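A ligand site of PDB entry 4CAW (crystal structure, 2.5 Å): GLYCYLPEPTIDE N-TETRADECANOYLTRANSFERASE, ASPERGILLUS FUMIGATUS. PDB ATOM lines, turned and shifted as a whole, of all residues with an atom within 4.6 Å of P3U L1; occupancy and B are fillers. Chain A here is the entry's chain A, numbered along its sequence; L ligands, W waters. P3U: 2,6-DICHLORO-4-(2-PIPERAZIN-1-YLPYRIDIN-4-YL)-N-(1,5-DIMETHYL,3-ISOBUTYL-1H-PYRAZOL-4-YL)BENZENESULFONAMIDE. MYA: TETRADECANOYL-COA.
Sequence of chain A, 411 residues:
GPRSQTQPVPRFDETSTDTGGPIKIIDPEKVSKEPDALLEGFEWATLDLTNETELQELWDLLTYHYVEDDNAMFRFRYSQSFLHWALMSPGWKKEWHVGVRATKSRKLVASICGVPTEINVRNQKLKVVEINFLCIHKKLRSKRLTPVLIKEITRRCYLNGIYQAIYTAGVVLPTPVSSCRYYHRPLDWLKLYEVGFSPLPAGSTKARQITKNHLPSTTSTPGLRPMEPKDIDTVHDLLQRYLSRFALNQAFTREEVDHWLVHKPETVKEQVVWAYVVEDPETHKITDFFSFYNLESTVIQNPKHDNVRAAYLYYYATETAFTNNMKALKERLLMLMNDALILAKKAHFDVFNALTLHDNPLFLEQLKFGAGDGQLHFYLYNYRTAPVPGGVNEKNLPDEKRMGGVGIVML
NAU of P3U L1 is in salt-bridge range of O of Leu 411 (2.8 Å).
The side-chain hydroxyl (OG) of Ser 297 sits at hydrogen-bond distance from a nitrogen (NAT) of P3U L1, 2.8 Å away.
A ring nitrogen (NE2) of His 184 sits at hydrogen-bond distance from an oxygen (OAE) of P3U L1 (3.5 Å).
The backbone NH (N) of Gly 170 is in hydrogen-bond range of a nitrogen (NAS) of P3U L1, at 3.4 Å.
The chain-end carboxylate of Leu 411 sits at hydrogen-bond distance from the side-chain amide nitrogen of Asn 132, 2.6 Å away.
A ring nitrogen (ND1) of His 184 sits at hydrogen-bond distance from the side-chain amide oxygen (OD1) of Asn 353, at 2.9 Å.
The side-chain carboxylate (OD1) of Asp 69 is in hydrogen-bond range of the backbone NH (N) of Phe 74 (2.9 Å).
The backbone carbonyl oxygen (O) of Val 67 sits at hydrogen-bond distance from the backbone NH (N) of Phe 76 (3.1 Å).
OG1 of Thr 168 lies close to SD of Met 410 (3.8 Å).
N of Tyr 182 is in hydrogen-bond range of O of Gly 374 (3.0 Å).
OD1 of Asn 132 lies within hydrogen-bond range of OH of Tyr 66 (3.2 Å).
The guanidinium group (NE) of Arg 75 lies within salt-bridge range of the side-chain carboxylate (OE2) of Glu 68 (2.7 Å).
Residues that only touch P3U L1: Val 67 (3.7 Å), Asp 69 (3.3 Å), Phe 74 (3.6 Å), Arg 75 (3.8 Å), Phe 76 (3.4 Å), Asn 132 (3.7 Å), Thr 168 (3.4 Å), Tyr 182 (3.5 Å), Phe 197 (3.5 Å), Val 308 (3.9 Å), Tyr 312 (3.0 Å), Val 351 (3.8 Å), Gly 374 (3.5 Å), Leu 376 (3.5 Å) and Met 410 (3.9 Å).
Hydrophobic or aromatic side chains that line P3U L1: Val 67, Phe 74, Phe 76, Tyr 182, His 184, Phe 197, Val 308, Tyr 312, Val 351 and Leu 376.
19 residues have an atom within 4 Å of P3U L1: Val 67, Asp 69, Phe 74, Arg 75, Phe 76, Asn 132, Thr 168, Gly 170, Tyr 182, His 184, Phe 197, Ser 297, Val 308, Tyr 312, Val 351, Gly 374, Leu 376, Met 410 and Leu 411.
Along chain A the residues within 4 Å of P3U L1 span positions 67 to 411.
Water W1 lies within hydrogen-bond range of N of Gly 170 (2.8 Å), NAS of P3U L1 (2.8 Å) and S1 of MYA L2 (3.4 Å).
Water W3 lies within hydrogen-bond range of OH of Tyr 66 (2.5 Å), OH of Tyr 78 (2.8 Å), NAU of P3U L1 (2.9 Å), OD1 of Asn 132 (2.9 Å) and O of Leu 411 (3.3 Å).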
ATOM      1  N   TYR A  66     -28.260  -5.851   1.237  1.00  0.00           N
ATOM      2  CA  TYR A  66     -27.300  -4.795   1.561  1.00  0.00           C
ATOM      3  C   TYR A  66     -26.406  -5.172   2.747  1.00  0.00           C
ATOM      4  O   TYR A  66     -26.379  -6.333   3.175  1.00  0.00           O
ATOM      5  CB  TYR A  66     -27.993  -3.443   1.757  1.00  0.00           C
ATOM      6  CG  TYR A  66     -27.092  -2.242   1.547  1.00  0.00           C
ATOM      7  CD1 TYR A  66     -26.267  -2.138   0.425  1.00  0.00           C
ATOM      8  CD2 TYR A  66     -27.074  -1.195   2.465  1.00  0.00           C
ATOM      9  CE1 TYR A  66     -25.444  -1.037   0.230  1.00  0.00           C
ATOM     10  CE2 TYR A  66     -26.251  -0.084   2.285  1.00  0.00           C
ATOM     11  CZ  TYR A  66     -25.439  -0.010   1.166  1.00  0.00           C
ATOM     12  OH  TYR A  66     -24.632   1.084   0.994  1.00  0.00           O
ATOM     13  N   VAL A  67     -25.677  -4.184   3.276  1.00  0.00           N
ATOM     14  CA  VAL A  67     -24.627  -4.396   4.278  1.00  0.00           C
ATOM     15  C   VAL A  67     -25.075  -5.208   5.496  1.00  0.00           C
ATOM     16  O   VAL A  67     -25.994  -4.835   6.215  1.00  0.00           O
ATOM     17  CB  VAL A  67     -24.013  -3.053   4.780  1.00  0.00           C
ATOM     18  CG1 VAL A  67     -22.843  -3.307   5.717  1.00  0.00           C
ATOM     19  CG2 VAL A  67     -23.562  -2.184   3.616  1.00  0.00           C
ATOM     20  N   GLU A  68     -24.409  -6.351   5.678  1.00  0.00           N
ATOM     21  CA  GLU A  68     -24.554  -7.158   6.880  1.00  0.00           C
ATOM     22  C   GLU A  68     -23.271  -7.050   7.704  1.00  0.00           C
ATOM     23  O   GLU A  68     -22.237  -6.619   7.189  1.00  0.00           O
ATOM     24  CB  GLU A  68     -24.820  -8.622   6.500  1.00  0.00           C
ATOM     25  CG  GLU A  68     -26.209  -8.889   5.916  1.00  0.00           C
ATOM     26  CD  GLU A  68     -26.467 -10.358   5.588  1.00  0.00           C
ATOM     27  OE1 GLU A  68     -25.744 -11.243   6.093  1.00  0.00           O
ATOM     28  OE2 GLU A  68     -27.411 -10.635   4.806  1.00  0.00           O
ATOM     29  N   ASP A  69     -23.337  -7.414   8.984  1.00  0.00           N
ATOM     30  CA  ASP A  69     -22.116  -7.657   9.748  1.00  0.00           C
ATOM     31  C   ASP A  69     -21.601  -9.047   9.395  1.00  0.00           C
ATOM     32  O   ASP A  69     -22.195  -9.737   8.562  1.00  0.00           O
ATOM     33  CB  ASP A  69     -22.345  -7.524  11.262  1.00  0.00           C
ATOM     34  CG  ASP A  69     -23.385  -8.486  11.801  1.00  0.00           C
ATOM     35  OD1 ASP A  69     -24.586  -8.286  11.530  1.00  0.00           O
ATOM     36  OD2 ASP A  69     -23.003  -9.447  12.513  1.00  0.00           O
ATOM     37  N   PHE A  74     -27.371  -8.999  11.663  1.00  0.00           N
ATOM     38  CA  PHE A  74     -27.889  -7.667  11.307  1.00  0.00           C
ATOM     39  C   PHE A  74     -27.696  -7.274   9.843  1.00  0.00           C
ATOM     40  O   PHE A  74     -26.717  -7.664   9.201  1.00  0.00           O
ATOM     41  CB  PHE A  74     -27.269  -6.583  12.204  1.00  0.00           C
ATOM     42  CG  PHE A  74     -27.363  -6.870  13.672  1.00  0.00           C
ATOM     43  CD1 PHE A  74     -28.561  -6.681  14.358  1.00  0.00           C
ATOM     44  CD2 PHE A  74     -26.259  -7.347  14.367  1.00  0.00           C
ATOM     45  CE1 PHE A  74     -28.648  -6.959  15.718  1.00  0.00           C
ATOM     46  CE2 PHE A  74     -26.345  -7.624  15.728  1.00  0.00           C
ATOM     47  CZ  PHE A  74     -27.541  -7.424  16.406  1.00  0.00           C
ATOM     48  N   ARG A  75     -28.654  -6.497   9.323  1.00  0.00           N
ATOM     49  CA  ARG A  75     -28.581  -5.933   7.972  1.00  0.00           C
ATOM     50  C   ARG A  75     -29.273  -4.566   7.955  1.00  0.00           C
ATOM     51  O   ARG A  75     -30.322  -4.402   8.574  1.00  0.00           O
ATOM     52  CB  ARG A  75     -29.236  -6.862   6.956  1.00  0.00           C
ATOM     53  CG  ARG A  75     -28.853  -6.559   5.511  1.00  0.00           C
ATOM     54  CD  ARG A  75     -29.626  -7.423   4.504  1.00  0.00           C
ATOM     55  NE  ARG A  75     -29.483  -8.858   4.759  1.00  0.00           N
ATOM     56  CZ  ARG A  75     -30.484  -9.668   5.104  1.00  0.00           C
ATOM     57  NH1 ARG A  75     -31.715  -9.186   5.261  1.00  0.00           N
ATOM     58  NH2 ARG A  75     -30.255 -10.952   5.307  1.00  0.00           N
ATOM     59  N   PHE A  76     -28.680  -3.603   7.251  1.00  0.00           N
ATOM     60  CA  PHE A  76     -29.261  -2.268   7.141  1.00  0.00           C
ATOM     61  C   PHE A  76     -30.620  -2.303   6.449  1.00  0.00           C
ATOM     62  O   PHE A  76     -30.789  -2.942   5.412  1.00  0.00           O
ATOM     63  CB  PHE A  76     -28.343  -1.304   6.391  1.00  0.00           C
ATOM     64  CG  PHE A  76     -27.168  -0.813   7.197  1.00  0.00           C
ATOM     65  CD1 PHE A  76     -27.267  -0.603   8.566  1.00  0.00           C
ATOM     66  CD2 PHE A  76     -25.951  -0.542   6.568  1.00  0.00           C
ATOM     67  CE1 PHE A  76     -26.176  -0.152   9.301  1.00  0.00           C
ATOM     68  CE2 PHE A  76     -24.859  -0.080   7.296  1.00  0.00           C
ATOM     69  CZ  PHE A  76     -24.973   0.114   8.673  1.00  0.00           C
ATOM     70  N   TYR A  78     -32.427   0.612   5.250  1.00  0.00           N
ATOM     71  CA  TYR A  78     -32.668   1.975   4.785  1.00  0.00           C
ATOM     72  C   TYR A  78     -34.120   2.071   4.317  1.00  0.00           C
ATOM     73  O   TYR A  78     -34.560   1.281   3.486  1.00  0.00           O
ATOM     74  CB  TYR A  78     -31.738   2.334   3.623  1.00  0.00           C
ATOM     75  CG  TYR A  78     -30.302   2.602   4.032  1.00  0.00           C
ATOM     76  CD1 TYR A  78     -29.889   3.885   4.375  1.00  0.00           C
ATOM     77  CD2 TYR A  78     -29.357   1.576   4.038  1.00  0.00           C
ATOM     78  CE1 TYR A  78     -28.562   4.146   4.731  1.00  0.00           C
ATOM     79  CE2 TYR A  78     -28.032   1.825   4.402  1.00  0.00           C
ATOM     80  CZ  TYR A  78     -27.642   3.108   4.749  1.00  0.00           C
ATOM     81  OH  TYR A  78     -26.341   3.360   5.109  1.00  0.00           O
ATOM     82  N   ASN A 132     -22.475   5.574  -3.122  1.00  0.00           N
ATOM     83  CA  ASN A 132     -23.139   4.838  -2.054  1.00  0.00           C
ATOM     84  C   ASN A 132     -24.109   3.797  -2.621  1.00  0.00           C
ATOM     85  O   ASN A 132     -24.407   3.798  -3.817  1.00  0.00           O
ATOM     86  CB  ASN A 132     -23.883   5.813  -1.121  1.00  0.00           C
ATOM     87  CG  ASN A 132     -24.048   5.275   0.293  1.00  0.00           C
ATOM     88  OD1 ASN A 132     -23.635   4.153   0.610  1.00  0.00           O
ATOM     89  ND2 ASN A 132     -24.672   6.069   1.152  1.00  0.00           N
ATOM     90  N   THR A 168     -17.348   5.826   1.105  1.00  0.00           N
ATOM     91  CA  THR A 168     -17.180   5.247   2.425  1.00  0.00           C
ATOM     92  C   THR A 168     -17.335   3.733   2.339  1.00  0.00           C
ATOM     93  O   THR A 168     -18.207   3.238   1.612  1.00  0.00           O
ATOM     94  CB  THR A 168     -18.189   5.909   3.392  1.00  0.00           C
ATOM     95  OG1 THR A 168     -17.516   6.905   4.178  1.00  0.00           O
ATOM     96  CG2 THR A 168     -18.821   4.909   4.300  1.00  0.00           C
ATOM     97  N   ALA A 169     -16.475   2.997   3.030  1.00  0.00           N
ATOM     98  CA  ALA A 169     -16.509   1.525   3.018  1.00  0.00           C
ATOM     99  C   ALA A 169     -15.951   0.909   4.296  1.00  0.00           C
ATOM    100  O   ALA A 169     -14.909   1.334   4.803  1.00  0.00           O
ATOM    101  CB  ALA A 169     -15.776   0.975   1.798  1.00  0.00           C
ATOM    102  N   GLY A 170     -16.638  -0.108   4.807  1.00  0.00           N
ATOM    103  CA  GLY A 170     -16.214  -0.820   6.015  1.00  0.00           C
ATOM    104  C   GLY A 170     -15.175  -1.901   5.770  1.00  0.00           C
ATOM    105  O   GLY A 170     -14.778  -2.604   6.704  1.00  0.00           O
ATOM    106  N   TYR A 182     -16.503   2.950  14.833  1.00  0.00           N
ATOM    107  CA  TYR A 182     -17.884   3.102  15.265  1.00  0.00           C
ATOM    108  C   TYR A 182     -18.016   3.084  16.787  1.00  0.00           C
ATOM    109  O   TYR A 182     -17.349   2.295  17.472  1.00  0.00           O
ATOM    110  CB  TYR A 182     -18.766   2.024  14.641  1.00  0.00           C
ATOM    111  CG  TYR A 182     -19.239   2.348  13.247  1.00  0.00           C
ATOM    112  CD1 TYR A 182     -20.327   3.196  13.046  1.00  0.00           C
ATOM    113  CD2 TYR A 182     -18.606   1.819  12.134  1.00  0.00           C
ATOM    114  CE1 TYR A 182     -20.771   3.513  11.761  1.00  0.00           C
ATOM    115  CE2 TYR A 182     -19.036   2.116  10.850  1.00  0.00           C
ATOM    116  CZ  TYR A 182     -20.114   2.965  10.669  1.00  0.00           C
ATOM    117  OH  TYR A 182     -20.553   3.276   9.403  1.00  0.00           O
ATOM    118  N   HIS A 184     -21.100   3.407  20.096  1.00  0.00           N
ATOM    119  CA  HIS A 184     -22.501   3.077  20.322  1.00  0.00           C
ATOM    120  C   HIS A 184     -22.970   3.360  21.741  1.00  0.00           C
ATOM    121  O   HIS A 184     -22.473   2.768  22.704  1.00  0.00           O
ATOM    122  CB  HIS A 184     -22.763   1.606  19.961  1.00  0.00           C
ATOM    123  CG  HIS A 184     -21.969   1.115  18.791  1.00  0.00           C
ATOM    124  ND1 HIS A 184     -22.236   1.508  17.503  1.00  0.00           N
ATOM    125  CD2 HIS A 184     -20.899   0.293  18.722  1.00  0.00           C
ATOM    126  CE1 HIS A 184     -21.369   0.941  16.681  1.00  0.00           C
ATOM    127  NE2 HIS A 184     -20.553   0.189  17.398  1.00  0.00           N
ATOM    128  N   LEU A 192     -30.714  -4.174  22.993  1.00  0.00           N
ATOM    129  CA  LEU A 192     -29.416  -4.458  22.368  1.00  0.00           C
ATOM    130  C   LEU A 192     -28.814  -5.774  22.852  1.00  0.00           C
ATOM    131  O   LEU A 192     -28.134  -6.473  22.102  1.00  0.00           O
ATOM    132  CB  LEU A 192     -28.434  -3.300  22.604  1.00  0.00           C
ATOM    133  CG  LEU A 192     -28.774  -1.897  22.111  1.00  0.00           C
ATOM    134  CD1 LEU A 192     -27.671  -0.929  22.510  1.00  0.00           C
ATOM    135  CD2 LEU A 192     -29.007  -1.838  20.604  1.00  0.00           C
ATOM    136  N   PHE A 197     -26.390  -7.600  20.305  1.00  0.00           N
ATOM    137  CA  PHE A 197     -25.448  -6.500  20.026  1.00  0.00           C
ATOM    138  C   PHE A 197     -24.596  -6.116  21.231  1.00  0.00           C
ATOM    139  O   PHE A 197     -23.379  -5.947  21.088  1.00  0.00           O
ATOM    140  CB  PHE A 197     -26.182  -5.267  19.467  1.00  0.00           C
ATOM    141  CG  PHE A 197     -25.249  -4.180  19.010  1.00  0.00           C
ATOM    142  CD1 PHE A 197     -24.512  -4.320  17.842  1.00  0.00           C
ATOM    143  CD2 PHE A 197     -25.105  -3.010  19.747  1.00  0.00           C
ATOM    144  CE1 PHE A 197     -23.645  -3.320  17.413  1.00  0.00           C
ATOM    145  CE2 PHE A 197     -24.247  -1.996  19.336  1.00  0.00           C
ATOM    146  CZ  PHE A 197     -23.507  -2.149  18.162  1.00  0.00           C
ATOM    147  N   SER A 297     -31.862  -1.264  11.394  1.00  0.00           N
ATOM    148  CA  SER A 297     -31.213  -2.528  11.077  1.00  0.00           C
ATOM    149  C   SER A 297     -32.142  -3.694  11.405  1.00  0.00           C
ATOM    150  O   SER A 297     -32.757  -3.728  12.469  1.00  0.00           O
ATOM    151  CB  SER A 297     -29.896  -2.683  11.828  1.00  0.00           C
ATOM    152  OG  SER A 297     -28.828  -2.093  11.101  1.00  0.00           O
ATOM    153  N   VAL A 308     -34.039  -3.346  14.863  1.00  0.00           N
ATOM    154  CA  VAL A 308     -33.352  -2.420  15.762  1.00  0.00           C
ATOM    155  C   VAL A 308     -33.367  -1.016  15.169  1.00  0.00           C
ATOM    156  O   VAL A 308     -32.907  -0.807  14.043  1.00  0.00           O
ATOM    157  CB  VAL A 308     -31.882  -2.859  16.044  1.00  0.00           C
ATOM    158  CG1 VAL A 308     -31.150  -1.801  16.871  1.00  0.00           C
ATOM    159  CG2 VAL A 308     -31.841  -4.188  16.756  1.00  0.00           C
ATOM    160  N   TYR A 312     -28.046   7.862  14.177  1.00  0.00           N
ATOM    161  CA  TYR A 312     -26.656   8.118  13.839  1.00  0.00           C
ATOM    162  C   TYR A 312     -26.362   9.615  13.907  1.00  0.00           C
ATOM    163  O   TYR A 312     -27.029  10.419  13.260  1.00  0.00           O
ATOM    164  CB  TYR A 312     -26.347   7.621  12.423  1.00  0.00           C
ATOM    165  CG  TYR A 312     -26.323   6.128  12.259  1.00  0.00           C
ATOM    166  CD1 TYR A 312     -27.499   5.372  12.295  1.00  0.00           C
ATOM    167  CD2 TYR A 312     -25.124   5.453  12.049  1.00  0.00           C
ATOM    168  CE1 TYR A 312     -27.475   3.994  12.141  1.00  0.00           C
ATOM    169  CE2 TYR A 312     -25.094   4.074  11.882  1.00  0.00           C
ATOM    170  CZ  TYR A 312     -26.272   3.352  11.931  1.00  0.00           C
ATOM    171  OH  TYR A 312     -26.245   1.986  11.769  1.00  0.00           O
ATOM    172  N   VAL A 351     -30.316   2.788  20.028  1.00  0.00           N
ATOM    173  CA  VAL A 351     -28.892   3.052  20.133  1.00  0.00           C
ATOM    174  C   VAL A 351     -28.515   4.291  19.331  1.00  0.00           C
ATOM    175  O   VAL A 351     -29.048   4.541  18.251  1.00  0.00           O
ATOM    176  CB  VAL A 351     -28.048   1.795  19.706  1.00  0.00           C
ATOM    177  CG1 VAL A 351     -28.237   1.485  18.216  1.00  0.00           C
ATOM    178  CG2 VAL A 351     -26.580   1.951  20.066  1.00  0.00           C
ATOM    179  N   ASN A 353     -25.534   5.919  17.402  1.00  0.00           N
ATOM    180  CA  ASN A 353     -24.253   5.614  16.763  1.00  0.00           C
ATOM    181  C   ASN A 353     -23.508   6.878  16.362  1.00  0.00           C
ATOM    182  O   ASN A 353     -24.113   7.858  15.919  1.00  0.00           O
ATOM    183  CB  ASN A 353     -24.437   4.693  15.559  1.00  0.00           C
ATOM    184  CG  ASN A 353     -24.989   3.335  15.933  1.00  0.00           C
ATOM    185  OD1 ASN A 353     -24.776   2.838  17.043  1.00  0.00           O
ATOM    186  ND2 ASN A 353     -25.700   2.712  15.000  1.00  0.00           N
ATOM    187  N   GLY A 374     -16.998  -2.357  14.444  1.00  0.00           N
ATOM    188  CA  GLY A 374     -17.087  -1.743  13.130  1.00  0.00           C
ATOM    189  C   GLY A 374     -16.090  -0.629  12.908  1.00  0.00           C
ATOM    190  O   GLY A 374     -15.827   0.176  13.809  1.00  0.00           O
ATOM    191  N   LEU A 376     -14.998   2.317   9.822  1.00  0.00           N
ATOM    192  CA  LEU A 376     -15.359   2.979   8.569  1.00  0.00           C
ATOM    193  C   LEU A 376     -14.163   3.695   7.945  1.00  0.00           C
ATOM    194  O   LEU A 376     -13.506   4.509   8.591  1.00  0.00           O
ATOM    195  CB  LEU A 376     -16.523   3.951   8.782  1.00  0.00           C
ATOM    196  CG  LEU A 376     -17.282   4.318   7.504  1.00  0.00           C
ATOM    197  CD1 LEU A 376     -18.082   3.129   7.006  1.00  0.00           C
ATOM    198  CD2 LEU A 376     -18.175   5.518   7.736  1.00  0.00           C
ATOM    199  N   MET A 410     -20.786  10.341   5.830  1.00  0.00           N
ATOM    200  CA  MET A 410     -21.417   9.699   4.684  1.00  0.00           C
ATOM    201  C   MET A 410     -22.429   8.646   5.139  1.00  0.00           C
ATOM    202  O   MET A 410     -22.152   7.872   6.065  1.00  0.00           O
ATOM    203  CB  MET A 410     -20.367   9.087   3.757  1.00  0.00           C
ATOM    204  CG  MET A 410     -19.414  10.112   3.164  1.00  0.00           C
ATOM    205  SD  MET A 410     -18.555   9.561   1.683  1.00  0.00           S
ATOM    206  CE  MET A 410     -19.908   9.456   0.516  1.00  0.00           C
ATOM    207  N   LEU A 411     -23.589   8.637   4.497  1.00  0.00           N
ATOM    208  CA  LEU A 411     -24.747   7.866   4.960  1.00  0.00           C
ATOM    209  C   LEU A 411     -24.617   6.348   4.739  1.00  0.00           C
ATOM    210  O   LEU A 411     -24.130   5.882   3.717  1.00  0.00           O
ATOM    211  CB  LEU A 411     -26.037   8.402   4.320  1.00  0.00           C
ATOM    212  CG  LEU A 411     -26.320   9.905   4.474  1.00  0.00           C
ATOM    213  CD1 LEU A 411     -27.425  10.345   3.536  1.00  0.00           C
ATOM    214  CD2 LEU A 411     -26.664  10.287   5.911  1.00  0.00           C
ATOM    215  OXT LEU A 411     -25.013   5.566   5.595  1.00  0.00           O
HETATM  216  CAP P3U L   1     -21.342   1.514   4.133  1.00  0.00           C
HETATM  217  CAN P3U L   1     -21.429   2.856   3.381  1.00  0.00           C
HETATM  218  NAU P3U L   1     -22.338   3.777   4.093  1.00  0.00           N
HETATM  219  CAO P3U L   1     -21.992   3.978   5.516  1.00  0.00           C
HETATM  220  CAQ P3U L   1     -21.882   2.628   6.248  1.00  0.00           C
HETATM  221  NBG P3U L   1     -20.898   1.770   5.530  1.00  0.00           N
HETATM  222  CBB P3U L   1     -20.590   0.576   6.217  1.00  0.00           C
HETATM  223  CAM P3U L   1     -20.962   0.385   7.558  1.00  0.00           C
HETATM  224  NAS P3U L   1     -19.901  -0.401   5.581  1.00  0.00           N
HETATM  225  CAI P3U L   1     -19.597  -1.549   6.177  1.00  0.00           C
HETATM  226  CAJ P3U L   1     -19.949  -1.785   7.507  1.00  0.00           C
HETATM  227  CAY P3U L   1     -20.640  -0.798   8.213  1.00  0.00           C
HETATM  228  CAZ P3U L   1     -21.013  -1.010   9.547  1.00  0.00           C
HETATM  229  CAL P3U L   1     -21.954  -0.187  10.153  1.00  0.00           C
HETATM  230  CAX P3U L   1     -22.342  -0.379  11.487  1.00  0.00           C
HETATM  231 CLH  P3U L   1     -23.519   0.697  12.146  1.00  0.00          CL
HETATM  232  CAK P3U L   1     -20.438  -2.043  10.294  1.00  0.00           C
HETATM  233  CAW P3U L   1     -20.809  -2.243  11.621  1.00  0.00           C
HETATM  234 CLG  P3U L   1     -20.060  -3.553  12.476  1.00  0.00          CL
HETATM  235  CBE P3U L   1     -21.753  -1.408  12.233  1.00  0.00           C
HETATM  236  SBI P3U L   1     -22.254  -1.698  13.918  1.00  0.00           S
HETATM  237  OAE P3U L   1     -21.075  -2.055  14.771  1.00  0.00           O
HETATM  238  OAF P3U L   1     -22.943  -0.495  14.496  1.00  0.00           O
HETATM  239  NAV P3U L   1     -23.318  -2.941  13.900  1.00  0.00           N
HETATM  240  CBD P3U L   1     -24.323  -2.982  13.012  1.00  0.00           C
HETATM  241  CBA P3U L   1     -24.351  -3.597  11.775  1.00  0.00           C
HETATM  242  CAA P3U L   1     -23.231  -4.377  11.097  1.00  0.00           C
HETATM  243  NBH P3U L   1     -25.559  -3.372  11.263  1.00  0.00           N
HETATM  244  CAD P3U L   1     -26.026  -3.854   9.930  1.00  0.00           C
HETATM  245  NAT P3U L   1     -26.257  -2.702  12.029  1.00  0.00           N
HETATM  246  CBC P3U L   1     -25.583  -2.419  13.151  1.00  0.00           C
HETATM  247  CAR P3U L   1     -26.123  -1.607  14.335  1.00  0.00           C
HETATM  248  CBF P3U L   1     -26.699  -2.506  15.431  1.00  0.00           C
HETATM  249  CAC P3U L   1     -26.896  -1.716  16.722  1.00  0.00           C
HETATM  250  CAB P3U L   1     -28.017  -3.157  15.005  1.00  0.00           C
HETATM  251  S1  MYA L   2     -19.938   0.669   0.488  1.00  0.00           S
HETATM  252  C2  MYA L   2     -21.118  -0.620   0.754  1.00  0.00           C
HETATM  253  C3  MYA L   2     -20.781  -1.789  -0.163  1.00  0.00           C
HETATM  254  N4  MYA L   2     -21.900  -2.711  -0.060  1.00  0.00           N
HETATM  255  C5  MYA L   2     -22.106  -3.698   0.805  1.00  0.00           C
HETATM  256  O5  MYA L   2     -21.341  -3.984   1.718  1.00  0.00           O
HETATM  257  C6  MYA L   2     -23.405  -4.459   0.606  1.00  0.00           C
HETATM  258  C7  MYA L   2     -23.239  -5.958   0.876  1.00  0.00           C
HETATM  259  N8  MYA L   2     -22.249  -6.462  -0.062  1.00  0.00           N
HETATM  260  C9  MYA L   2     -22.391  -6.738  -1.365  1.00  0.00           C
HETATM  261  O9  MYA L   2     -23.442  -6.608  -1.960  1.00  0.00           O
HETATM  262  C10 MYA L   2     -21.184  -7.276  -2.084  1.00  0.00           C
HETATM  263  O10 MYA L   2     -20.401  -8.066  -1.175  1.00  0.00           O
HETATM  264  C11 MYA L   2     -20.300  -6.206  -2.753  1.00  0.00           C
HETATM  265  C12 MYA L   2     -19.145  -6.887  -3.490  1.00  0.00           C
HETATM  266  C13 MYA L   2     -19.689  -5.253  -1.728  1.00  0.00           C
HETATM  267  C14 MYA L   2     -21.087  -5.400  -3.774  1.00  0.00           C
HETATM  268  N1A MYA L   2     -16.614  -1.030  -1.890  1.00  0.00           N
HETATM  269  O1A MYA L   2     -16.787 -10.425  -6.960  1.00  0.00           O
HETATM  270  P1A MYA L   2     -17.228  -9.032  -6.601  1.00  0.00           P
HETATM  271  C1X MYA L   2     -14.350  -5.003  -4.317  1.00  0.00           C
HETATM  272  C2A MYA L   2     -15.940  -1.029  -3.057  1.00  0.00           C
HETATM  273  O2A MYA L   2     -18.415  -8.414  -7.289  1.00  0.00           O
HETATM  274  P2A MYA L   2     -18.894  -9.371  -4.359  1.00  0.00           P
HETATM  275  C2M MYA L   2     -20.371   1.590  -0.838  1.00  0.00           C
HETATM  276  O2M MYA L   2     -21.519   1.587  -1.230  1.00  0.00           O
HETATM  277  C2X MYA L   2     -13.089  -5.761  -3.917  1.00  0.00           C
HETATM  278  O2X MYA L   2     -11.967  -4.887  -3.875  1.00  0.00           O
HETATM  279  N3A MYA L   2     -15.408  -2.162  -3.549  1.00  0.00           N
HETATM  280  O3A MYA L   2     -17.466  -8.995  -5.000  1.00  0.00           O
HETATM  281  C3M MYA L   2     -19.323   2.431  -1.533  1.00  0.00           C
HETATM  282  C3X MYA L   2     -12.928  -6.817  -4.991  1.00  0.00           C
HETATM  283  O3X MYA L   2     -11.844  -6.477  -5.847  1.00  0.00           O
HETATM  284  P3X MYA L   2     -10.467  -7.310  -5.765  1.00  0.00           P
HETATM  285  C4A MYA L   2     -15.545  -3.333  -2.877  1.00  0.00           C
HETATM  286  O4A MYA L   2     -19.621 -10.286  -5.309  1.00  0.00           O
HETATM  287  C4M MYA L   2     -19.137   1.937  -2.962  1.00  0.00           C
HETATM  288  C4X MYA L   2     -14.210  -6.788  -5.798  1.00  0.00           C
HETATM  289  O4X MYA L   2     -15.103  -5.886  -5.140  1.00  0.00           O
HETATM  290  C5A MYA L   2     -16.237  -3.356  -1.670  1.00  0.00           C
HETATM  291  O5A MYA L   2     -18.664  -9.808  -2.936  1.00  0.00           O
HETATM  292  C5M MYA L   2     -17.747   2.262  -3.493  1.00  0.00           C
HETATM  293  C5X MYA L   2     -14.835  -8.165  -5.916  1.00  0.00           C
HETATM  294  O5X MYA L   2     -15.955  -8.082  -6.796  1.00  0.00           O
HETATM  295  C6A MYA L   2     -16.771  -2.174  -1.182  1.00  0.00           C
HETATM  296  N6A MYA L   2     -17.454  -2.171  -0.011  1.00  0.00           N
HETATM  297  O6A MYA L   2     -19.621  -7.934  -4.341  1.00  0.00           O
HETATM  298  C6M MYA L   2     -17.586   1.875  -4.965  1.00  0.00           C
HETATM  299  N7A MYA L   2     -16.216  -4.626  -1.216  1.00  0.00           N
HETATM  300  O7A MYA L   2     -10.777  -8.865  -5.948  1.00  0.00           O
HETATM  301  C7M MYA L   2     -16.232   2.344  -5.521  1.00  0.00           C
HETATM  302  C8A MYA L   2     -15.538  -5.372  -2.114  1.00  0.00           C
HETATM  303  O8A MYA L   2      -9.475  -6.822  -6.927  1.00  0.00           O
HETATM  304  C8M MYA L   2     -16.234   3.850  -5.773  1.00  0.00           C
HETATM  305  N9A MYA L   2     -15.132  -4.584  -3.122  1.00  0.00           N
HETATM  306  O9A MYA L   2      -9.777  -7.060  -4.341  1.00  0.00           O
HETATM  307  C9M MYA L   2     -15.244   4.261  -6.853  1.00  0.00           C
HETATM  308  CAM MYA L   2     -15.590   5.650  -7.372  1.00  0.00           C
HETATM  309  CBM MYA L   2     -16.433   5.572  -8.651  1.00  0.00           C
HETATM  310  CCM MYA L   2     -16.923   6.944  -9.097  1.00  0.00           C
HETATM  311  CDM MYA L   2     -15.879   7.651  -9.961  1.00  0.00           C
HETATM  312  CEM MYA L   2     -16.522   8.771 -10.770  1.00  0.00           C
HETATM  313  CFM MYA L   2     -15.547   9.900 -11.002  1.00  0.00           C
HETATM  314  O   HOH W   1     -18.669  -0.989   3.133  1.00  0.00           O
HETATM  315  O   HOH W   2     -22.226  -5.298  14.308  1.00  0.00           O
HETATM  316  O   HOH W   3     -24.754   2.735   2.901  1.00  0.00           O
